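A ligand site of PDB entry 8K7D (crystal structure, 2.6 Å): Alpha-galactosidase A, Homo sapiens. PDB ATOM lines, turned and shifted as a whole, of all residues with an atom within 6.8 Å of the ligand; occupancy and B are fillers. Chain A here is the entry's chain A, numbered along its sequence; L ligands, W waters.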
ATOM      1  N   LEU A  14     -26.002  13.454  -0.463  1.00  0.00           N
ATOM      2  CA  LEU A  14     -26.561  14.679   0.099  1.00  0.00           C
ATOM      3  C   LEU A  14     -27.529  15.286  -0.918  1.00  0.00           C
ATOM      4  O   LEU A  14     -27.193  15.374  -2.102  1.00  0.00           O
ATOM      5  CB  LEU A  14     -25.444  15.676   0.435  1.00  0.00           C
ATOM      6  CG  LEU A  14     -25.795  16.985   1.161  1.00  0.00           C
ATOM      7  CD1 LEU A  14     -26.463  16.702   2.495  1.00  0.00           C
ATOM      8  CD2 LEU A  14     -24.545  17.826   1.343  1.00  0.00           C
ATOM      9  N   TRP A  16     -28.778  18.287  -1.511  1.00  0.00           N
ATOM     10  CA  TRP A  16     -28.952  19.722  -1.737  1.00  0.00           C
ATOM     11  C   TRP A  16     -28.877  20.092  -3.221  1.00  0.00           C
ATOM     12  O   TRP A  16     -29.803  20.719  -3.751  1.00  0.00           O
ATOM     13  CB  TRP A  16     -27.904  20.525  -0.955  1.00  0.00           C
ATOM     14  CG  TRP A  16     -28.166  21.975  -1.101  1.00  0.00           C
ATOM     15  CD1 TRP A  16     -27.399  22.887  -1.759  1.00  0.00           C
ATOM     16  CD2 TRP A  16     -29.323  22.689  -0.639  1.00  0.00           C
ATOM     17  NE1 TRP A  16     -27.986  24.130  -1.706  1.00  0.00           N
ATOM     18  CE2 TRP A  16     -29.166  24.034  -1.025  1.00  0.00           C
ATOM     19  CE3 TRP A  16     -30.458  22.320   0.072  1.00  0.00           C
ATOM     20  CZ2 TRP A  16     -30.110  25.005  -0.723  1.00  0.00           C
ATOM     21  CZ3 TRP A  16     -31.395  23.290   0.381  1.00  0.00           C
ATOM     22  CH2 TRP A  16     -31.221  24.612  -0.013  1.00  0.00           C
ATOM     23  N   ASP A  61     -29.982  17.723   3.962  1.00  0.00           N
ATOM     24  CA  ASP A  61     -29.522  19.114   3.998  1.00  0.00           C
ATOM     25  C   ASP A  61     -30.639  20.002   4.538  1.00  0.00           C
ATOM     26  O   ASP A  61     -31.463  19.547   5.330  1.00  0.00           O
ATOM     27  CB  ASP A  61     -29.086  19.561   2.602  1.00  0.00           C
ATOM     28  CG  ASP A  61     -27.997  20.614   2.643  1.00  0.00           C
ATOM     29  OD1 ASP A  61     -28.309  21.776   2.977  1.00  0.00           O
ATOM     30  OD2 ASP A  61     -26.837  20.285   2.341  1.00  0.00           O
ATOM     31  N   ASP A  62     -30.664  21.259   4.121  1.00  0.00           N
ATOM     32  CA  ASP A  62     -31.634  22.203   4.664  1.00  0.00           C
ATOM     33  C   ASP A  62     -33.052  21.830   4.238  1.00  0.00           C
ATOM     34  O   ASP A  62     -33.271  20.970   3.380  1.00  0.00           O
ATOM     35  CB  ASP A  62     -31.305  23.629   4.231  1.00  0.00           C
ATOM     36  CG  ASP A  62     -31.868  24.681   5.173  1.00  0.00           C
ATOM     37  OD1 ASP A  62     -32.680  24.324   6.044  1.00  0.00           O
ATOM     38  OD2 ASP A  62     -31.474  25.860   5.046  1.00  0.00           O
ATOM     39  N   CYS A  63     -34.029  22.470   4.891  1.00  0.00           N
ATOM     40  CA  CYS A  63     -35.454  22.362   4.553  1.00  0.00           C
ATOM     41  C   CYS A  63     -36.042  21.013   4.968  1.00  0.00           C
ATOM     42  O   CYS A  63     -36.823  20.405   4.221  1.00  0.00           O
ATOM     43  CB  CYS A  63     -35.704  22.648   3.072  1.00  0.00           C
ATOM     44  SG  CYS A  63     -34.932  24.199   2.562  1.00  0.00           S
ATOM     45  N   TYR A 103     -28.914  18.266   9.106  1.00  0.00           N
ATOM     46  CA  TYR A 103     -28.436  19.614   8.837  1.00  0.00           C
ATOM     47  C   TYR A 103     -28.883  20.563   9.943  1.00  0.00           C
ATOM     48  O   TYR A 103     -29.989  20.423  10.493  1.00  0.00           O
ATOM     49  CB  TYR A 103     -28.945  20.119   7.478  1.00  0.00           C
ATOM     50  CG  TYR A 103     -28.768  21.593   7.199  1.00  0.00           C
ATOM     51  CD1 TYR A 103     -29.708  22.521   7.649  1.00  0.00           C
ATOM     52  CD2 TYR A 103     -27.703  22.066   6.435  1.00  0.00           C
ATOM     53  CE1 TYR A 103     -29.561  23.868   7.390  1.00  0.00           C
ATOM     54  CE2 TYR A 103     -27.570  23.415   6.162  1.00  0.00           C
ATOM     55  CZ  TYR A 103     -28.500  24.311   6.640  1.00  0.00           C
ATOM     56  OH  TYR A 103     -28.369  25.650   6.382  1.00  0.00           O
ATOM     57  N   ASP A 105     -27.804  24.912  11.513  1.00  0.00           N
ATOM     58  CA  ASP A 105     -27.093  26.157  11.271  1.00  0.00           C
ATOM     59  C   ASP A 105     -26.604  26.753  12.585  1.00  0.00           C
ATOM     60  O   ASP A 105     -27.284  26.657  13.617  1.00  0.00           O
ATOM     61  CB  ASP A 105     -27.979  27.164  10.539  1.00  0.00           C
ATOM     62  CG  ASP A 105     -27.186  28.295   9.911  1.00  0.00           C
ATOM     63  OD1 ASP A 105     -26.620  29.103  10.659  1.00  0.00           O
ATOM     64  OD2 ASP A 105     -27.143  28.365   8.665  1.00  0.00           O
ATOM     65  N   THR A 110     -31.437  29.010   9.642  1.00  0.00           N
ATOM     66  CA  THR A 110     -30.778  28.318   8.553  1.00  0.00           C
ATOM     67  C   THR A 110     -30.820  29.196   7.304  1.00  0.00           C
ATOM     68  O   THR A 110     -31.541  30.199   7.246  1.00  0.00           O
ATOM     69  CB  THR A 110     -31.454  26.968   8.269  1.00  0.00           C
ATOM     70  OG1 THR A 110     -32.744  27.182   7.676  1.00  0.00           O
ATOM     71  CG2 THR A 110     -31.613  26.166   9.553  1.00  0.00           C
ATOM     72  N   CYS A 111     -30.029  28.825   6.299  1.00  0.00           N
ATOM     73  CA  CYS A 111     -29.970  29.623   5.075  1.00  0.00           C
ATOM     74  C   CYS A 111     -31.322  29.708   4.390  1.00  0.00           C
ATOM     75  O   CYS A 111     -31.624  30.710   3.731  1.00  0.00           O
ATOM     76  CB  CYS A 111     -28.915  29.073   4.123  1.00  0.00           C
ATOM     77  SG  CYS A 111     -27.195  29.126   4.741  1.00  0.00           S
ATOM     78  N   ALA A 112     -32.163  28.679   4.547  1.00  0.00           N
ATOM     79  CA  ALA A 112     -33.513  28.712   3.995  1.00  0.00           C
ATOM     80  C   ALA A 112     -34.514  29.415   4.891  1.00  0.00           C
ATOM     81  O   ALA A 112     -35.667  29.594   4.483  1.00  0.00           O
ATOM     82  CB  ALA A 112     -34.001  27.287   3.719  1.00  0.00           C
ATOM     83  N   GLY A 113     -34.129  29.807   6.100  1.00  0.00           N
ATOM     84  CA  GLY A 113     -34.996  30.537   6.991  1.00  0.00           C
ATOM     85  C   GLY A 113     -35.684  29.711   8.051  1.00  0.00           C
ATOM     86  O   GLY A 113     -36.700  30.155   8.604  1.00  0.00           O
ATOM     87  N   LYS A 137     -24.195  18.250   9.296  1.00  0.00           N
ATOM     88  CA  LYS A 137     -23.709  19.345   8.486  1.00  0.00           C
ATOM     89  C   LYS A 137     -24.150  20.650   9.130  1.00  0.00           C
ATOM     90  O   LYS A 137     -25.345  20.885   9.333  1.00  0.00           O
ATOM     91  CB  LYS A 137     -24.239  19.265   7.052  1.00  0.00           C
ATOM     92  CG  LYS A 137     -23.633  20.329   6.138  1.00  0.00           C
ATOM     93  CD  LYS A 137     -24.231  20.302   4.742  1.00  0.00           C
ATOM     94  CE  LYS A 137     -23.656  21.422   3.887  1.00  0.00           C
ATOM     95  NZ  LYS A 137     -24.416  21.627   2.619  1.00  0.00           N
ATOM     96  N   ASP A 139     -24.198  24.683   9.041  1.00  0.00           N
ATOM     97  CA  ASP A 139     -24.117  25.821   8.152  1.00  0.00           C
ATOM     98  C   ASP A 139     -23.817  27.104   8.935  1.00  0.00           C
ATOM     99  O   ASP A 139     -23.830  27.121  10.167  1.00  0.00           O
ATOM    100  CB  ASP A 139     -25.428  25.949   7.374  1.00  0.00           C
ATOM    101  CG  ASP A 139     -25.219  26.458   5.965  1.00  0.00           C
ATOM    102  OD1 ASP A 139     -24.130  26.975   5.654  1.00  0.00           O
ATOM    103  OD2 ASP A 139     -26.167  26.328   5.166  1.00  0.00           O
ATOM    104  N   GLY A 140     -23.560  28.190   8.203  1.00  0.00           N
ATOM    105  CA  GLY A 140     -23.117  29.418   8.839  1.00  0.00           C
ATOM    106  C   GLY A 140     -23.880  30.675   8.481  1.00  0.00           C
ATOM    107  O   GLY A 140     -23.335  31.775   8.575  1.00  0.00           O
ATOM    108  N   CYS A 141     -25.148  30.539   8.074  1.00  0.00           N
ATOM    109  CA  CYS A 141     -25.956  31.702   7.744  1.00  0.00           C
ATOM    110  C   CYS A 141     -26.458  32.395   9.006  1.00  0.00           C
ATOM    111  O   CYS A 141     -26.556  31.808  10.078  1.00  0.00           O
ATOM    112  CB  CYS A 141     -27.155  31.313   6.865  1.00  0.00           C
ATOM    113  SG  CYS A 141     -26.810  31.087   5.097  1.00  0.00           S
ATOM    114  N   GLU A 172     -18.984  24.402   7.826  1.00  0.00           N
ATOM    115  CA  GLU A 172     -18.834  25.397   6.764  1.00  0.00           C
ATOM    116  C   GLU A 172     -18.078  26.630   7.263  1.00  0.00           C
ATOM    117  O   GLU A 172     -18.093  27.672   6.588  1.00  0.00           O
ATOM    118  CB  GLU A 172     -20.195  25.807   6.196  1.00  0.00           C
ATOM    119  CG  GLU A 172     -20.952  24.687   5.500  1.00  0.00           C
ATOM    120  CD  GLU A 172     -21.821  25.184   4.358  1.00  0.00           C
ATOM    121  OE1 GLU A 172     -21.397  26.148   3.676  1.00  0.00           O
ATOM    122  OE2 GLU A 172     -22.912  24.630   4.153  1.00  0.00           O
ATOM    123  N   LEU A 175     -15.512  28.670   4.890  1.00  0.00           N
ATOM    124  CA  LEU A 175     -16.213  29.371   3.816  1.00  0.00           C
ATOM    125  C   LEU A 175     -16.816  30.686   4.310  1.00  0.00           C
ATOM    126  O   LEU A 175     -16.775  31.688   3.598  1.00  0.00           O
ATOM    127  CB  LEU A 175     -17.293  28.471   3.225  1.00  0.00           C
ATOM    128  CG  LEU A 175     -18.271  29.170   2.280  1.00  0.00           C
ATOM    129  CD1 LEU A 175     -17.534  29.694   1.067  1.00  0.00           C
ATOM    130  CD2 LEU A 175     -19.394  28.236   1.860  1.00  0.00           C
ATOM    131  N   TYR A 176     -17.365  30.687   5.516  1.00  0.00           N
ATOM    132  CA  TYR A 176     -17.938  31.915   6.050  1.00  0.00           C
ATOM    133  C   TYR A 176     -16.902  32.792   6.741  1.00  0.00           C
ATOM    134  O   TYR A 176     -17.234  33.906   7.160  1.00  0.00           O
ATOM    135  CB  TYR A 176     -19.063  31.594   7.023  1.00  0.00           C
ATOM    136  CG  TYR A 176     -20.329  31.114   6.357  1.00  0.00           C
ATOM    137  CD1 TYR A 176     -20.509  29.766   6.079  1.00  0.00           C
ATOM    138  CD2 TYR A 176     -21.339  31.998   6.009  1.00  0.00           C
ATOM    139  CE1 TYR A 176     -21.667  29.317   5.467  1.00  0.00           C
ATOM    140  CE2 TYR A 176     -22.489  31.558   5.390  1.00  0.00           C
ATOM    141  CZ  TYR A 176     -22.652  30.217   5.126  1.00  0.00           C
ATOM    142  OH  TYR A 176     -23.801  29.777   4.521  1.00  0.00           O
ATOM    143  N   ARG A 196     -16.094  22.965   4.599  1.00  0.00           N
ATOM    144  CA  ARG A 196     -16.313  23.590   3.311  1.00  0.00           C
ATOM    145  C   ARG A 196     -15.440  24.836   3.162  1.00  0.00           C
ATOM    146  O   ARG A 196     -15.461  25.719   4.029  1.00  0.00           O
ATOM    147  CB  ARG A 196     -17.792  23.948   3.149  1.00  0.00           C
ATOM    148  CG  ARG A 196     -18.684  22.769   2.804  1.00  0.00           C
ATOM    149  CD  ARG A 196     -18.585  22.434   1.332  1.00  0.00           C
ATOM    150  NE  ARG A 196     -18.781  23.621   0.510  1.00  0.00           N
ATOM    151  CZ  ARG A 196     -19.963  24.171   0.263  1.00  0.00           C
ATOM    152  NH1 ARG A 196     -21.078  23.637   0.717  1.00  0.00           N
ATOM    153  NH2 ARG A 196     -20.018  25.282  -0.473  1.00  0.00           N
ATOM    154  N   PHE A 198     -14.967  26.658  -0.215  1.00  0.00           N
ATOM    155  CA  PHE A 198     -15.298  27.547  -1.334  1.00  0.00           C
ATOM    156  C   PHE A 198     -16.803  27.534  -1.569  1.00  0.00           C
ATOM    157  O   PHE A 198     -17.560  26.803  -0.916  1.00  0.00           O
ATOM    158  CB  PHE A 198     -14.518  27.118  -2.587  1.00  0.00           C
ATOM    159  CG  PHE A 198     -14.627  28.089  -3.733  1.00  0.00           C
ATOM    160  CD1 PHE A 198     -14.127  29.370  -3.629  1.00  0.00           C
ATOM    161  CD2 PHE A 198     -15.240  27.697  -4.921  1.00  0.00           C
ATOM    162  CE1 PHE A 198     -14.226  30.257  -4.684  1.00  0.00           C
ATOM    163  CE2 PHE A 198     -15.339  28.584  -5.976  1.00  0.00           C
ATOM    164  CZ  PHE A 198     -14.832  29.864  -5.851  1.00  0.00           C
ATOM    165  N   ALA A 199     -17.250  28.381  -2.501  1.00  0.00           N
ATOM    166  CA  ALA A 199     -18.664  28.566  -2.780  1.00  0.00           C
ATOM    167  C   ALA A 199     -19.337  27.256  -3.190  1.00  0.00           C
ATOM    168  O   ALA A 199     -18.684  26.288  -3.596  1.00  0.00           O
ATOM    169  CB  ALA A 199     -18.853  29.601  -3.887  1.00  0.00           C
ATOM    170  N   ASP A 200     -20.659  27.239  -3.064  1.00  0.00           N
ATOM    171  CA  ASP A 200     -21.442  26.061  -3.405  1.00  0.00           C
ATOM    172  C   ASP A 200     -21.233  25.655  -4.860  1.00  0.00           C
ATOM    173  O   ASP A 200     -20.984  26.489  -5.736  1.00  0.00           O
ATOM    174  CB  ASP A 200     -22.935  26.308  -3.164  1.00  0.00           C
ATOM    175  CG  ASP A 200     -23.262  26.624  -1.722  1.00  0.00           C
ATOM    176  OD1 ASP A 200     -22.458  26.251  -0.838  1.00  0.00           O
ATOM    177  OD2 ASP A 200     -24.315  27.238  -1.476  1.00  0.00           O
ATOM    178  N   ASP A 235     -17.091  20.394  -1.893  1.00  0.00           N
ATOM    179  CA  ASP A 235     -18.523  20.266  -2.125  1.00  0.00           C
ATOM    180  C   ASP A 235     -18.840  19.017  -2.942  1.00  0.00           C
ATOM    181  O   ASP A 235     -17.947  18.249  -3.283  1.00  0.00           O
ATOM    182  CB  ASP A 235     -19.101  21.532  -2.793  1.00  0.00           C
ATOM    183  CG  ASP A 235     -20.524  21.816  -2.356  1.00  0.00           C
ATOM    184  OD1 ASP A 235     -21.074  21.007  -1.583  1.00  0.00           O
ATOM    185  OD2 ASP A 235     -21.069  22.861  -2.780  1.00  0.00           O
ATOM    186  N   MET A 236     -20.127  18.834  -3.264  1.00  0.00           N
ATOM    187  CA  MET A 236     -20.673  17.552  -3.671  1.00  0.00           C
ATOM    188  C   MET A 236     -20.236  17.125  -5.076  1.00  0.00           C
ATOM    189  O   MET A 236     -19.774  17.930  -5.889  1.00  0.00           O
ATOM    190  CB  MET A 236     -22.200  17.603  -3.622  1.00  0.00           C
ATOM    191  CG  MET A 236     -22.741  18.191  -2.339  1.00  0.00           C
ATOM    192  SD  MET A 236     -24.497  18.518  -2.408  1.00  0.00           S
ATOM    193  CE  MET A 236     -24.496  20.267  -2.757  1.00  0.00           C
HETATM  194  C1  LIG L   1     -26.440  24.364   1.545  1.00  0.00           C
HETATM  195  C2  LIG L   1     -28.509  25.024   2.764  1.00  0.00           C
HETATM  196  C3  LIG L   1     -25.197  25.118   1.146  1.00  0.00           C
HETATM  197  C4  LIG L   1     -25.135  26.178   2.238  1.00  0.00           C
HETATM  198  C5  LIG L   1     -24.416  27.433   1.741  1.00  0.00           C
HETATM  199  C6  LIG L   1     -27.375  25.505   1.856  1.00  0.00           C
HETATM  200  N1  LIG L   1     -26.536  26.479   2.583  1.00  0.00           N
HETATM  201  N2  LIG L   1     -22.958  27.292   1.821  1.00  0.00           N
HETATM  202  O1  LIG L   1     -26.183  23.610   2.753  1.00  0.00           O
HETATM  203  O2  LIG L   1     -24.047  24.260   1.221  1.00  0.00           O
HETATM  204  O3  LIG L   1     -29.441  26.085   2.954  1.00  0.00           O
HETATM  205  O   HOH W   1     -27.619  29.119   1.146  1.00  0.00           O
HETATM  206  O   HOH W   2     -22.320  30.420   1.495  1.00  0.00           O
HETATM  207  O   HOH W   3     -23.505  23.213  -1.850  1.00  0.00           O
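Water W1 lies within hydrogen-bond range of N1 of the ligand and SG of Cys 111. Water W2 lies within hydrogen-bond range of N2 of the ligand (3.2 Å) and OH of Tyr 176 (3.4 Å). Water W3 lies within hydrogen-bond range of the side-chain carboxylate of Asp 235, an oxygen (O2) of the ligand and the side-chain carboxylate of Asp 200.
N2 of the ligand is in salt-bridge range of OD1 of Asp 200 (2.9 Å). The guanidinium group of Arg 196 lies within hydrogen-bond range of an oxygen (O2) of the ligand. OD2 of Asp 139 is in salt-bridge range of N1 of the ligand (2.6 Å). O1 of the ligand is in hydrogen-bond range of NZ of Lys 137 (2.7 Å). The side-chain carboxylate (OD2) of Asp 62 lies within hydrogen-bond range of an oxygen (O3) of the ligand (2.9 Å). OD1 of Asp 61 is in hydrogen-bond range of O1 of the ligand (2.8 Å). A nitrogen (N2) of the ligand lies within salt-bridge range of the side-chain carboxylate of Glu 172, at 2.7 Å. The side-chain sulfur (SG) of Cys 111 lies within hydrogen-bond range of a nitrogen (N1) of the ligand.
Merely in contact with the ligand: Trp 16, Tyr 103, Leu 175 and Tyr 176. Hydrophobic or aromatic side chains that line the ligand: Trp 16, Tyr 103 and Leu 175.
The side-chain carboxylate of Glu 172 is in salt-bridge range of the side-chain amino group of Lys 137 (3.7 Å). The side-chain sulfur of Cys 111 is disulfide-bonded to the side-chain sulfur of Cys 141 (2.0 Å). OD2 of Asp 139 lies within hydrogen-bond range of OH of Tyr 103 (2.6 Å). The backbone carbonyl oxygen of Arg 196 lies within hydrogen-bond range of the backbone NH of Leu 175 (3.1 Å). OH of Tyr 176 is in hydrogen-bond range of SG of Cys 111, at 3.5 Å. The guanidinium group of Arg 196 lies within hydrogen-bond range of the backbone carbonyl oxygen of Phe 198. The side-chain carboxylate (OE1) of Glu 172 lies within salt-bridge range of the guanidinium group (NH1) of Arg 196, 3.9 Å away. NH2 of Arg 196 lies within salt-bridge range of OD1 of Asp 200, at 2.7 Å.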
